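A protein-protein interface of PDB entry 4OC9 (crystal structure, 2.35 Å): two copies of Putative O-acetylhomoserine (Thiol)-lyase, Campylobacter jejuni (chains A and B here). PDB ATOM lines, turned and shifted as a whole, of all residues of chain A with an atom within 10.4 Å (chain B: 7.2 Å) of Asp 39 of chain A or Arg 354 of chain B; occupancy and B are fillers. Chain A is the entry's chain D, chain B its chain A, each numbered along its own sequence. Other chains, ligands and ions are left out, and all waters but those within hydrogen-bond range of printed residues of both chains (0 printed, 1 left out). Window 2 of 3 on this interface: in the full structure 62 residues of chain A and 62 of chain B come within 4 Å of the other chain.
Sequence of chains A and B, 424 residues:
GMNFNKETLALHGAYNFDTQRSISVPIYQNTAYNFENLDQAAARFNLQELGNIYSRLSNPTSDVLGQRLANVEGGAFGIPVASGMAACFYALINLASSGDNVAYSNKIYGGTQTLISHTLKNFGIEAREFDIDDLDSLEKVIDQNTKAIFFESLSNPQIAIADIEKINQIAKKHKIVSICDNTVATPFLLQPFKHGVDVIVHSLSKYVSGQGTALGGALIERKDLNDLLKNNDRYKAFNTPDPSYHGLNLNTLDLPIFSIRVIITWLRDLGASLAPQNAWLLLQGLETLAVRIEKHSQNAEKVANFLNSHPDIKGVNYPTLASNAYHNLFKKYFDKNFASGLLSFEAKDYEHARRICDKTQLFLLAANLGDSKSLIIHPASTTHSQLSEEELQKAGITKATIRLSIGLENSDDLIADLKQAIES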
ATOM      1  N   PHE A  35      29.047   9.025 -12.565  1.00  0.00           N
ATOM      2  CA  PHE A  35      29.963   9.903 -13.267  1.00  0.00           C
ATOM      3  C   PHE A  35      29.873  11.237 -12.555  1.00  0.00           C
ATOM      4  O   PHE A  35      28.790  11.639 -12.129  1.00  0.00           O
ATOM      5  CB  PHE A  35      29.591  10.079 -14.723  1.00  0.00           C
ATOM      6  CG  PHE A  35      29.473   8.787 -15.456  1.00  0.00           C
ATOM      7  CD1 PHE A  35      30.613   8.032 -15.742  1.00  0.00           C
ATOM      8  CD2 PHE A  35      28.252   8.335 -15.884  1.00  0.00           C
ATOM      9  CE1 PHE A  35      30.515   6.836 -16.397  1.00  0.00           C
ATOM     10  CE2 PHE A  35      28.159   7.131 -16.563  1.00  0.00           C
ATOM     11  CZ  PHE A  35      29.284   6.394 -16.823  1.00  0.00           C
ATOM     12  N   GLU A  36      31.013  11.925 -12.423  1.00  0.00           N
ATOM     13  CA  GLU A  36      31.080  13.233 -11.725  1.00  0.00           C
ATOM     14  C   GLU A  36      30.422  14.365 -12.527  1.00  0.00           C
ATOM     15  O   GLU A  36      30.013  15.363 -11.944  1.00  0.00           O
ATOM     16  CB  GLU A  36      32.513  13.619 -11.392  1.00  0.00           C
ATOM     17  CG  GLU A  36      33.263  12.569 -10.587  1.00  0.00           C
ATOM     18  CD  GLU A  36      34.688  12.963 -10.306  1.00  0.00           C
ATOM     19  OE1 GLU A  36      34.923  14.118  -9.919  1.00  0.00           O
ATOM     20  OE2 GLU A  36      35.576  12.094 -10.413  1.00  0.00           O
ATOM     21  N   ASN A  37      30.323  14.206 -13.844  1.00  0.00           N
ATOM     22  CA  ASN A  37      29.697  15.210 -14.707  1.00  0.00           C
ATOM     23  C   ASN A  37      29.490  14.617 -16.075  1.00  0.00           C
ATOM     24  O   ASN A  37      30.039  13.566 -16.385  1.00  0.00           O
ATOM     25  CB  ASN A  37      30.542  16.458 -14.760  1.00  0.00           C
ATOM     26  CG  ASN A  37      31.904  16.205 -15.329  1.00  0.00           C
ATOM     27  OD1 ASN A  37      32.053  15.514 -16.339  1.00  0.00           O
ATOM     28  ND2 ASN A  37      32.914  16.827 -14.732  1.00  0.00           N
ATOM     29  N   LEU A  38      28.686  15.267 -16.894  1.00  0.00           N
ATOM     30  CA  LEU A  38      28.413  14.739 -18.242  1.00  0.00           C
ATOM     31  C   LEU A  38      29.631  14.590 -19.160  1.00  0.00           C
ATOM     32  O   LEU A  38      29.719  13.631 -19.927  1.00  0.00           O
ATOM     33  CB  LEU A  38      27.302  15.512 -18.943  1.00  0.00           C
ATOM     34  CG  LEU A  38      26.726  14.745 -20.170  1.00  0.00           C
ATOM     35  CD1 LEU A  38      25.863  13.728 -19.456  1.00  0.00           C
ATOM     36  CD2 LEU A  38      25.836  15.497 -21.155  1.00  0.00           C
ATOM     37  N   ASP A  39      30.579  15.511 -19.089  1.00  0.00           N
ATOM     38  CA  ASP A  39      31.780  15.414 -19.938  1.00  0.00           C
ATOM     39  C   ASP A  39      32.528  14.140 -19.654  1.00  0.00           C
ATOM     40  O   ASP A  39      32.904  13.403 -20.577  1.00  0.00           O
ATOM     41  CB  ASP A  39      32.739  16.597 -19.710  1.00  0.00           C
ATOM     42  CG  ASP A  39      32.173  17.933 -20.188  1.00  0.00           C
ATOM     43  OD1 ASP A  39      31.169  17.949 -20.928  1.00  0.00           O
ATOM     44  OD2 ASP A  39      32.783  18.962 -19.836  1.00  0.00           O
ATOM     45  N   GLN A  40      32.767  13.904 -18.366  1.00  0.00           N
ATOM     46  CA  GLN A  40      33.477  12.719 -17.924  1.00  0.00           C
ATOM     47  C   GLN A  40      32.852  11.452 -18.508  1.00  0.00           C
ATOM     48  O   GLN A  40      33.551  10.565 -18.994  1.00  0.00           O
ATOM     49  CB  GLN A  40      33.407  12.605 -16.418  1.00  0.00           C
ATOM     50  CG  GLN A  40      34.252  11.467 -15.872  1.00  0.00           C
ATOM     51  CD  GLN A  40      34.150  11.343 -14.357  1.00  0.00           C
ATOM     52  OE1 GLN A  40      33.080  11.150 -13.812  1.00  0.00           O
ATOM     53  NE2 GLN A  40      35.288  11.351 -13.689  1.00  0.00           N
ATOM     54  N   ALA A  41      31.529  11.374 -18.401  1.00  0.00           N
ATOM     55  CA  ALA A  41      30.784  10.235 -18.895  1.00  0.00           C
ATOM     56  C   ALA A  41      31.036  10.042 -20.391  1.00  0.00           C
ATOM     57  O   ALA A  41      31.616   9.057 -20.811  1.00  0.00           O
ATOM     58  CB  ALA A  41      29.309  10.422 -18.604  1.00  0.00           C
ATOM     59  N   ALA A  42      30.630  11.023 -21.179  1.00  0.00           N
ATOM     60  CA  ALA A  42      30.813  10.983 -22.631  1.00  0.00           C
ATOM     61  C   ALA A  42      32.268  10.691 -22.993  1.00  0.00           C
ATOM     62  O   ALA A  42      32.543   9.914 -23.896  1.00  0.00           O
ATOM     63  CB  ALA A  42      30.353  12.299 -23.274  1.00  0.00           C
ATOM     64  N   ALA A  43      33.195  11.312 -22.290  1.00  0.00           N
ATOM     65  CA  ALA A  43      34.587  11.083 -22.573  1.00  0.00           C
ATOM     66  C   ALA A  43      34.933   9.603 -22.400  1.00  0.00           C
ATOM     67  O   ALA A  43      35.735   9.063 -23.162  1.00  0.00           O
ATOM     68  CB  ALA A  43      35.464  11.966 -21.703  1.00  0.00           C
ATOM     69  N   ARG A  44      34.347   8.941 -21.400  1.00  0.00           N
ATOM     70  CA  ARG A  44      34.618   7.504 -21.185  1.00  0.00           C
ATOM     71  C   ARG A  44      33.986   6.658 -22.274  1.00  0.00           C
ATOM     72  O   ARG A  44      34.568   5.668 -22.693  1.00  0.00           O
ATOM     73  CB  ARG A  44      34.191   7.014 -19.806  1.00  0.00           C
ATOM     74  CG  ARG A  44      35.043   7.589 -18.709  1.00  0.00           C
ATOM     75  CD  ARG A  44      34.611   7.126 -17.341  1.00  0.00           C
ATOM     76  NE  ARG A  44      35.413   7.808 -16.339  1.00  0.00           N
ATOM     77  CZ  ARG A  44      35.206   7.738 -15.027  1.00  0.00           C
ATOM     78  NH1 ARG A  44      34.201   7.026 -14.519  1.00  0.00           N
ATOM     79  NH2 ARG A  44      36.007   8.396 -14.220  1.00  0.00           N
ATOM     80  N   PHE A  45      32.785   7.023 -22.707  1.00  0.00           N
ATOM     81  CA  PHE A  45      32.128   6.273 -23.786  1.00  0.00           C
ATOM     82  C   PHE A  45      32.850   6.401 -25.126  1.00  0.00           C
ATOM     83  O   PHE A  45      32.630   5.574 -26.011  1.00  0.00           O
ATOM     84  CB  PHE A  45      30.670   6.666 -23.941  1.00  0.00           C
ATOM     85  CG  PHE A  45      29.785   6.111 -22.887  1.00  0.00           C
ATOM     86  CD1 PHE A  45      29.637   6.726 -21.672  1.00  0.00           C
ATOM     87  CD2 PHE A  45      29.068   4.956 -23.137  1.00  0.00           C
ATOM     88  CE1 PHE A  45      28.795   6.190 -20.714  1.00  0.00           C
ATOM     89  CE2 PHE A  45      28.213   4.420 -22.193  1.00  0.00           C
ATOM     90  CZ  PHE A  45      28.075   5.041 -20.979  1.00  0.00           C
ATOM     91  N   ASN A  46      33.724   7.403 -25.255  1.00  0.00           N
ATOM     92  CA  ASN A  46      34.519   7.660 -26.481  1.00  0.00           C
ATOM     93  C   ASN A  46      35.960   7.210 -26.401  1.00  0.00           C
ATOM     94  O   ASN A  46      36.744   7.486 -27.299  1.00  0.00           O
ATOM     95  CB  ASN A  46      34.613   9.138 -26.740  1.00  0.00           C
ATOM     96  CG  ASN A  46      33.279   9.758 -26.986  1.00  0.00           C
ATOM     97  OD1 ASN A  46      32.322   9.087 -27.384  1.00  0.00           O
ATOM     98  ND2 ASN A  46      33.213  11.063 -26.797  1.00  0.00           N
ATOM     99  N   LEU A  47      36.315   6.527 -25.332  1.00  0.00           N
ATOM    100  CA  LEU A  47      37.689   6.051 -25.153  1.00  0.00           C
ATOM    101  C   LEU A  47      38.701   7.193 -25.010  1.00  0.00           C
ATOM    102  O   LEU A  47      39.896   6.950 -25.046  1.00  0.00           O
ATOM    103  CB  LEU A  47      38.154   5.033 -26.213  1.00  0.00           C
ATOM    104  CG  LEU A  47      37.411   3.702 -26.285  1.00  0.00           C
ATOM    105  CD1 LEU A  47      35.974   3.846 -26.787  1.00  0.00           C
ATOM    106  CD2 LEU A  47      38.184   2.802 -27.233  1.00  0.00           C
ATOM    107  N   GLN A  48      38.225   8.424 -24.837  1.00  0.00           N
ATOM    108  CA  GLN A  48      39.153   9.528 -24.649  1.00  0.00           C
ATOM    109  C   GLN A  48      39.709   9.397 -23.234  1.00  0.00           C
ATOM    110  O   GLN A  48      40.912   9.452 -23.044  1.00  0.00           O
ATOM    111  CB  GLN A  48      38.532  10.885 -24.931  1.00  0.00           C
ATOM    112  CG  GLN A  48      38.164  11.047 -26.396  1.00  0.00           C
ATOM    113  CD  GLN A  48      37.633  12.423 -26.724  1.00  0.00           C
ATOM    114  OE1 GLN A  48      37.606  13.308 -25.870  1.00  0.00           O
ATOM    115  NE2 GLN A  48      37.226  12.618 -27.975  1.00  0.00           N
ATOM    116  N   GLU A  49      38.846   9.151 -22.255  1.00  0.00           N
ATOM    117  CA  GLU A  49      39.308   8.983 -20.876  1.00  0.00           C
ATOM    118  C   GLU A  49      39.039   7.561 -20.394  1.00  0.00           C
ATOM    119  O   GLU A  49      37.966   7.016 -20.636  1.00  0.00           O
ATOM    120  CB  GLU A  49      38.592   9.913 -19.862  1.00  0.00           C
ATOM    121  CG  GLU A  49      38.597  11.436 -20.037  1.00  0.00           C
ATOM    122  CD  GLU A  49      37.810  12.152 -18.911  1.00  0.00           C
ATOM    123  OE1 GLU A  49      37.606  13.400 -18.945  1.00  0.00           O
ATOM    124  OE2 GLU A  49      37.381  11.451 -17.966  1.00  0.00           O
ATOM    125  N   LEU A  50      40.016   6.935 -19.751  1.00  0.00           N
ATOM    126  CA  LEU A  50      39.783   5.584 -19.204  1.00  0.00           C
ATOM    127  C   LEU A  50      39.145   5.640 -17.823  1.00  0.00           C
ATOM    128  O   LEU A  50      39.413   6.555 -17.054  1.00  0.00           O
ATOM    129  CB  LEU A  50      40.993   4.672 -19.179  1.00  0.00           C
ATOM    130  CG  LEU A  50      41.006   4.182 -20.641  1.00  0.00           C
ATOM    131  CD1 LEU A  50      41.781   5.207 -21.438  1.00  0.00           C
ATOM    132  CD2 LEU A  50      41.622   2.811 -20.849  1.00  0.00           C
ATOM    133  N   ASN A  52      35.769   3.802 -14.994  1.00  0.00           N
ATOM    134  CA  ASN A  52      34.567   3.012 -14.753  1.00  0.00           C
ATOM    135  C   ASN A  52      33.370   3.500 -15.502  1.00  0.00           C
ATOM    136  O   ASN A  52      33.089   4.705 -15.547  1.00  0.00           O
ATOM    137  CB  ASN A  52      34.215   3.022 -13.277  1.00  0.00           C
ATOM    138  CG  ASN A  52      35.307   2.432 -12.422  1.00  0.00           C
ATOM    139  OD1 ASN A  52      36.167   1.711 -12.915  1.00  0.00           O
ATOM    140  ND2 ASN A  52      35.252   2.709 -11.127  1.00  0.00           N
ATOM    141  N   ILE A  53      32.650   2.543 -16.071  1.00  0.00           N
ATOM    142  CA  ILE A  53      31.442   2.823 -16.843  1.00  0.00           C
ATOM    143  C   ILE A  53      30.270   1.923 -16.447  1.00  0.00           C
ATOM    144  O   ILE A  53      29.243   2.398 -15.963  1.00  0.00           O
ATOM    145  CB  ILE A  53      31.675   2.608 -18.347  1.00  0.00           C
ATOM    146  CG1 ILE A  53      32.706   3.587 -18.877  1.00  0.00           C
ATOM    147  CG2 ILE A  53      30.368   2.790 -19.096  1.00  0.00           C
ATOM    148  CD1 ILE A  53      33.062   3.391 -20.355  1.00  0.00           C
ATOM    149  N   ALA B 347      14.782  18.395 -23.333  1.00  0.00           N
ATOM    150  CA  ALA B 347      15.134  19.626 -22.627  1.00  0.00           C
ATOM    151  C   ALA B 347      15.026  20.719 -23.682  1.00  0.00           C
ATOM    152  O   ALA B 347      14.707  20.417 -24.828  1.00  0.00           O
ATOM    153  CB  ALA B 347      16.559  19.554 -22.104  1.00  0.00           C
ATOM    154  N   ASP B 349      17.360  22.446 -25.070  1.00  0.00           N
ATOM    155  CA  ASP B 349      18.417  22.182 -26.027  1.00  0.00           C
ATOM    156  C   ASP B 349      19.573  21.413 -25.356  1.00  0.00           C
ATOM    157  O   ASP B 349      19.511  21.090 -24.159  1.00  0.00           O
ATOM    158  CB  ASP B 349      18.907  23.508 -26.591  1.00  0.00           C
ATOM    159  CG  ASP B 349      19.368  24.467 -25.506  1.00  0.00           C
ATOM    160  OD1 ASP B 349      19.720  24.021 -24.401  1.00  0.00           O
ATOM    161  OD2 ASP B 349      19.407  25.683 -25.783  1.00  0.00           O
ATOM    162  N   TYR B 350      20.617  21.128 -26.129  1.00  0.00           N
ATOM    163  CA  TYR B 350      21.781  20.416 -25.637  1.00  0.00           C
ATOM    164  C   TYR B 350      22.359  21.019 -24.341  1.00  0.00           C
ATOM    165  O   TYR B 350      22.570  20.309 -23.363  1.00  0.00           O
ATOM    166  CB  TYR B 350      22.860  20.304 -26.724  1.00  0.00           C
ATOM    167  CG  TYR B 350      24.123  19.696 -26.169  1.00  0.00           C
ATOM    168  CD1 TYR B 350      24.221  18.327 -25.972  1.00  0.00           C
ATOM    169  CD2 TYR B 350      25.202  20.487 -25.815  1.00  0.00           C
ATOM    170  CE1 TYR B 350      25.342  17.752 -25.421  1.00  0.00           C
ATOM    171  CE2 TYR B 350      26.338  19.926 -25.284  1.00  0.00           C
ATOM    172  CZ  TYR B 350      26.412  18.552 -25.093  1.00  0.00           C
ATOM    173  OH  TYR B 350      27.562  17.981 -24.551  1.00  0.00           O
ATOM    174  N   GLU B 351      22.601  22.322 -24.321  1.00  0.00           N
ATOM    175  CA  GLU B 351      23.153  22.967 -23.120  1.00  0.00           C
ATOM    176  C   GLU B 351      22.274  22.820 -21.872  1.00  0.00           C
ATOM    177  O   GLU B 351      22.788  22.723 -20.761  1.00  0.00           O
ATOM    178  CB  GLU B 351      23.483  24.451 -23.381  1.00  0.00           C
ATOM    179  CG  GLU B 351      24.653  24.684 -24.348  1.00  0.00           C
ATOM    180  CD  GLU B 351      26.024  24.249 -23.792  1.00  0.00           C
ATOM    181  OE1 GLU B 351      26.210  24.230 -22.546  1.00  0.00           O
ATOM    182  OE2 GLU B 351      26.942  23.975 -24.605  1.00  0.00           O
ATOM    183  N   HIS B 352      20.957  22.810 -22.058  1.00  0.00           N
ATOM    184  CA  HIS B 352      20.030  22.666 -20.941  1.00  0.00           C
ATOM    185  C   HIS B 352      20.071  21.216 -20.448  1.00  0.00           C
ATOM    186  O   HIS B 352      20.105  20.975 -19.256  1.00  0.00           O
ATOM    187  CB  HIS B 352      18.628  23.137 -21.364  1.00  0.00           C
ATOM    188  CG  HIS B 352      17.605  23.140 -20.263  1.00  0.00           C
ATOM    189  ND1 HIS B 352      16.378  22.521 -20.382  1.00  0.00           N
ATOM    190  CD2 HIS B 352      17.656  23.627 -19.001  1.00  0.00           C
ATOM    191  CE1 HIS B 352      15.700  22.671 -19.261  1.00  0.00           C
ATOM    192  NE2 HIS B 352      16.462  23.321 -18.399  1.00  0.00           N
ATOM    193  N   ALA B 353      20.127  20.260 -21.376  1.00  0.00           N
ATOM    194  CA  ALA B 353      20.172  18.840 -21.035  1.00  0.00           C
ATOM    195  C   ALA B 353      21.404  18.491 -20.209  1.00  0.00           C
ATOM    196  O   ALA B 353      21.367  17.655 -19.302  1.00  0.00           O
ATOM    197  CB  ALA B 353      20.159  18.000 -22.291  1.00  0.00           C
ATOM    198  N   ARG B 354      22.480  19.202 -20.492  1.00  0.00           N
ATOM    199  CA  ARG B 354      23.733  19.008 -19.835  1.00  0.00           C
ATOM    200  C   ARG B 354      23.680  19.665 -18.439  1.00  0.00           C
ATOM    201  O   ARG B 354      24.149  19.095 -17.454  1.00  0.00           O
ATOM    202  CB  ARG B 354      24.807  19.674 -20.703  1.00  0.00           C
ATOM    203  CG  ARG B 354      26.225  19.194 -20.607  1.00  0.00           C
ATOM    204  CD  ARG B 354      27.163  20.259 -21.172  1.00  0.00           C
ATOM    205  NE  ARG B 354      27.493  21.421 -20.361  1.00  0.00           N
ATOM    206  CZ  ARG B 354      28.589  21.587 -19.628  1.00  0.00           C
ATOM    207  NH1 ARG B 354      29.527  20.656 -19.583  1.00  0.00           N
ATOM    208  NH2 ARG B 354      28.744  22.724 -18.946  1.00  0.00           N
ATOM    209  N   ARG B 355      23.092  20.843 -18.323  1.00  0.00           N
ATOM    210  CA  ARG B 355      23.013  21.540 -17.053  1.00  0.00           C
ATOM    211  C   ARG B 355      22.178  20.665 -16.056  1.00  0.00           C
ATOM    212  O   ARG B 355      22.502  20.513 -14.854  1.00  0.00           O
ATOM    213  CB  ARG B 355      22.435  22.969 -17.347  1.00  0.00           C
ATOM    214  CG  ARG B 355      22.675  24.055 -16.316  1.00  0.00           C
ATOM    215  CD  ARG B 355      22.612  25.448 -17.020  1.00  0.00           C
ATOM    216  NE  ARG B 355      21.343  25.705 -17.692  1.00  0.00           N
ATOM    217  CZ  ARG B 355      21.080  25.842 -19.008  1.00  0.00           C
ATOM    218  NH1 ARG B 355      22.030  25.973 -19.936  1.00  0.00           N
ATOM    219  NH2 ARG B 355      19.812  26.029 -19.387  1.00  0.00           N
ATOM    220  N   ILE B 356      21.123  20.044 -16.576  1.00  0.00           N
ATOM    221  CA  ILE B 356      20.244  19.165 -15.781  1.00  0.00           C
ATOM    222  C   ILE B 356      21.045  17.986 -15.262  1.00  0.00           C
ATOM    223  O   ILE B 356      21.036  17.708 -14.067  1.00  0.00           O
ATOM    224  CB  ILE B 356      19.056  18.670 -16.603  1.00  0.00           C
ATOM    225  CG1 ILE B 356      18.121  19.843 -16.923  1.00  0.00           C
ATOM    226  CG2 ILE B 356      18.267  17.644 -15.811  1.00  0.00           C
ATOM    227  CD1 ILE B 356      17.000  19.483 -17.882  1.00  0.00           C
ATOM    228  N   CYS B 357      21.747  17.297 -16.152  1.00  0.00           N
ATOM    229  CA  CYS B 357      22.570  16.161 -15.723  1.00  0.00           C
ATOM    230  C   CYS B 357      23.623  16.535 -14.677  1.00  0.00           C
ATOM    231  O   CYS B 357      23.926  15.732 -13.803  1.00  0.00           O
ATOM    232  CB  CYS B 357      23.304  15.527 -16.896  1.00  0.00           C
ATOM    233  SG  CYS B 357      22.213  14.732 -18.094  1.00  0.00           S
ATOM    234  N   ASP B 358      24.162  17.747 -14.769  1.00  0.00           N
ATOM    235  CA  ASP B 358      25.177  18.216 -13.839  1.00  0.00           C
ATOM    236  C   ASP B 358      24.614  18.796 -12.511  1.00  0.00           C
ATOM    237  O   ASP B 358      25.362  18.950 -11.545  1.00  0.00           O
ATOM    238  CB  ASP B 358      26.094  19.236 -14.546  1.00  0.00           C
ATOM    239  CG  ASP B 358      26.932  18.625 -15.718  1.00  0.00           C
ATOM    240  OD1 ASP B 358      26.970  17.386 -15.940  1.00  0.00           O
ATOM    241  OD2 ASP B 358      27.576  19.407 -16.458  1.00  0.00           O
ATOM    242  N   LYS B 359      23.301  19.059 -12.453  1.00  0.00           N
ATOM    243  CA  LYS B 359      22.619  19.638 -11.260  1.00  0.00           C
ATOM    244  C   LYS B 359      21.788  18.717 -10.367  1.00  0.00           C
ATOM    245  O   LYS B 359      21.545  19.077  -9.209  1.00  0.00           O
ATOM    246  CB  LYS B 359      21.727  20.799 -11.692  1.00  0.00           C
ATOM    247  CG  LYS B 359      22.449  22.057 -12.178  1.00  0.00           C
ATOM    248  CD  LYS B 359      23.085  22.856 -11.056  1.00  0.00           C
ATOM    249  CE  LYS B 359      21.992  23.479 -10.193  1.00  0.00           C
ATOM    250  NZ  LYS B 359      22.487  24.274  -9.036  1.00  0.00           N
ATOM    251  N   LEU B 365      23.872  10.548 -11.993  1.00  0.00           N
ATOM    252  CA  LEU B 365      24.364  10.508 -13.354  1.00  0.00           C
ATOM    253  C   LEU B 365      25.112   9.201 -13.482  1.00  0.00           C
ATOM    254  O   LEU B 365      26.201   9.040 -12.936  1.00  0.00           O
ATOM    255  CB  LEU B 365      25.299  11.667 -13.614  1.00  0.00           C
ATOM    256  CG  LEU B 365      25.893  11.688 -15.032  1.00  0.00           C
ATOM    257  CD1 LEU B 365      24.800  11.707 -16.087  1.00  0.00           C
ATOM    258  CD2 LEU B 365      26.810  12.894 -15.193  1.00  0.00           C
ATOM    259  N   HIS B 378      22.305  11.208 -20.612  1.00  0.00           N
ATOM    260  CA  HIS B 378      22.099  11.877 -21.912  1.00  0.00           C
ATOM    261  C   HIS B 378      22.541  10.888 -23.018  1.00  0.00           C
ATOM    262  O   HIS B 378      23.711  10.881 -23.394  1.00  0.00           O
ATOM    263  CB  HIS B 378      22.979  13.119 -21.987  1.00  0.00           C
ATOM    264  CG  HIS B 378      22.826  13.880 -23.257  1.00  0.00           C
ATOM    265  ND1 HIS B 378      23.448  13.500 -24.432  1.00  0.00           N
ATOM    266  CD2 HIS B 378      22.155  15.025 -23.530  1.00  0.00           C
ATOM    267  CE1 HIS B 378      23.137  14.363 -25.381  1.00  0.00           C
ATOM    268  NE2 HIS B 378      22.355  15.295 -24.862  1.00  0.00           N
ATOM    269  N   SER B 381      25.354  11.143 -26.433  1.00  0.00           N
ATOM    270  CA  SER B 381      26.804  11.081 -26.142  1.00  0.00           C
ATOM    271  C   SER B 381      27.203   9.943 -25.190  1.00  0.00           C
ATOM    272  O   SER B 381      28.341   9.887 -24.680  1.00  0.00           O
ATOM    273  CB  SER B 381      27.208  12.393 -25.452  1.00  0.00           C
ATOM    274  OG  SER B 381      26.599  12.521 -24.161  1.00  0.00           O
ATOM    275  N   LYS B 399      19.705  15.731 -29.457  1.00  0.00           N
ATOM    276  CA  LYS B 399      20.754  16.272 -28.589  1.00  0.00           C
ATOM    277  C   LYS B 399      20.193  16.832 -27.289  1.00  0.00           C
ATOM    278  O   LYS B 399      20.936  17.107 -26.336  1.00  0.00           O
ATOM    279  CB  LYS B 399      21.573  17.367 -29.301  1.00  0.00           C
ATOM    280  CG  LYS B 399      22.655  16.875 -30.262  1.00  0.00           C
ATOM    281  CD  LYS B 399      23.376  17.929 -31.105  1.00  0.00           C
ATOM    282  CE  LYS B 399      24.007  19.095 -30.361  1.00  0.00           C
ATOM    283  NZ  LYS B 399      25.259  18.826 -29.621  1.00  0.00           N
ATOM    284  N   ALA B 400      18.882  17.036 -27.257  1.00  0.00           N
ATOM    285  CA  ALA B 400      18.219  17.574 -26.076  1.00  0.00           C
ATOM    286  C   ALA B 400      17.579  16.465 -25.223  1.00  0.00           C
ATOM    287  O   ALA B 400      17.073  16.731 -24.136  1.00  0.00           O
ATOM    288  CB  ALA B 400      17.151  18.580 -26.511  1.00  0.00           C
ATOM    289  N   ILE B 402      16.917  13.401 -22.740  1.00  0.00           N
ATOM    290  CA  ILE B 402      17.372  12.923 -21.430  1.00  0.00           C
ATOM    291  C   ILE B 402      16.580  11.707 -21.086  1.00  0.00           C
ATOM    292  O   ILE B 402      15.378  11.679 -21.307  1.00  0.00           O
ATOM    293  CB  ILE B 402      17.167  13.959 -20.329  1.00  0.00           C
ATOM    294  CG1 ILE B 402      18.238  15.018 -20.452  1.00  0.00           C
ATOM    295  CG2 ILE B 402      17.348  13.317 -18.950  1.00  0.00           C
ATOM    296  CD1 ILE B 402      18.096  16.162 -19.488  1.00  0.00           C
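No position is printed for both chains. Of the 9 pairs that touch across the chains among the printed residues, none has its exchanged pair printed and touching as well.
Asn 37 of chain A touches Asp 358 of chain B. Asn 37 of chain A touches Leu 365 of chain B. Leu 38 of chain A touches Arg 354 of chain B (CD2 to CG, 3.8 Å). Leu 38 of chain A touches Leu 365 of chain B (N to CD2, 3.5 Å). His 378 of chain B touches Leu 38 of chain A. Ala 42 of chain A touches Ser 381 of chain B.
The side-chain carboxylate (OD2) of Asp 358 of chain B is in salt-bridge range of the guanidinium group (NH1) of Arg 354 of chain B. The backbone NH of Gln 40 of chain A is in hydrogen-bond range of the side-chain amide oxygen of Asn 37 of chain A. N of Asp 39 of chain A sits at hydrogen-bond distance from OD1 of Asn 37 of chain A, 3.1 Å away. O of Lys 399 of chain B is in hydrogen-bond range of NE2 of His 378 of chain B (2.7 Å). O of Ala 42 of chain A sits close to ND2 of Asn 46 of chain A (3.2 Å). The side-chain carboxylate (OE1) of Glu 351 of chain B is in salt-bridge range of the guanidinium group (NE) of Arg 354 of chain B (3.8 Å).
Printed residues of chain B that touch a printed residue of chain A: Arg 354, Asp 358, Leu 365, His 378 and Ser 381. Hydrophobic or aromatic side chains of chain B that line the printed part of chain A: Leu 365 and His 378. Of the 18 printed residues of chain A, 5 touch a printed residue of chain B. Along chain A the printed residues that touch a printed residue of chain B span positions 35 to 42. Among the printed residues, 9 pairs touch across the chains. Among the printed residues, Asp or Glu carboxylates within 4 Å of a Lys or Arg side-chain nitrogen of the other chain: Asp 39 of chain A with Arg 354 of chain B.
NH1 of Arg 354 of chain B is in salt-bridge range of OD1 of Asp 39 of chain A (3.4 Å). N of Leu 38 of chain A lies within hydrogen-bond range of OD1 of Asp 358 of chain B (2.9 Å). The backbone carbonyl oxygen of Leu 365 of chain B sits at hydrogen-bond distance from the backbone NH of Phe 35 of chain A (2.9 Å).
Asp 39 of chain A touches one residue of chain B. Arg 354 of chain B touches just these residues of chain A: Leu 38 and Asp 39. No residue of chain A comes within 4 Å of Tyr 350 of chain B. No residue of chain A comes within 4 Å of Glu 351 of chain B. No residue of chain A comes within 4 Å of Ala 353 of chain B. No residue of chain A comes within 4 Å of Cys 357 of chain B. Of chain A, only Asn 37 (3.7 Å) and Leu 38 (2.9 Å) come within 4 Å of Asp 358 of chain B. Printed residues of chain B within 4 Å of Ala 42 of chain A: Ser 381 (3.4 Å). Of the printed residues of chain B, Asn 37 of chain A touches Asp 358 (3.7 Å) and Leu 365 (3.3 Å). Glu 36 of chain A touches none of the printed residues of chain B. Asn 46 of chain A touches none of the printed residues of chain B. The nearest residue of chain B that does not touch Asp 39 of chain A is Tyr 350 of chain B (5.1 Å). The nearest residue of chain A that does not touch Arg 354 of chain B is Asn 37 of chain A (6.5 Å). The nearest printed residue of chain B that does not touch Phe 35 of chain A is Cys 357 of chain B (6.6 Å).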
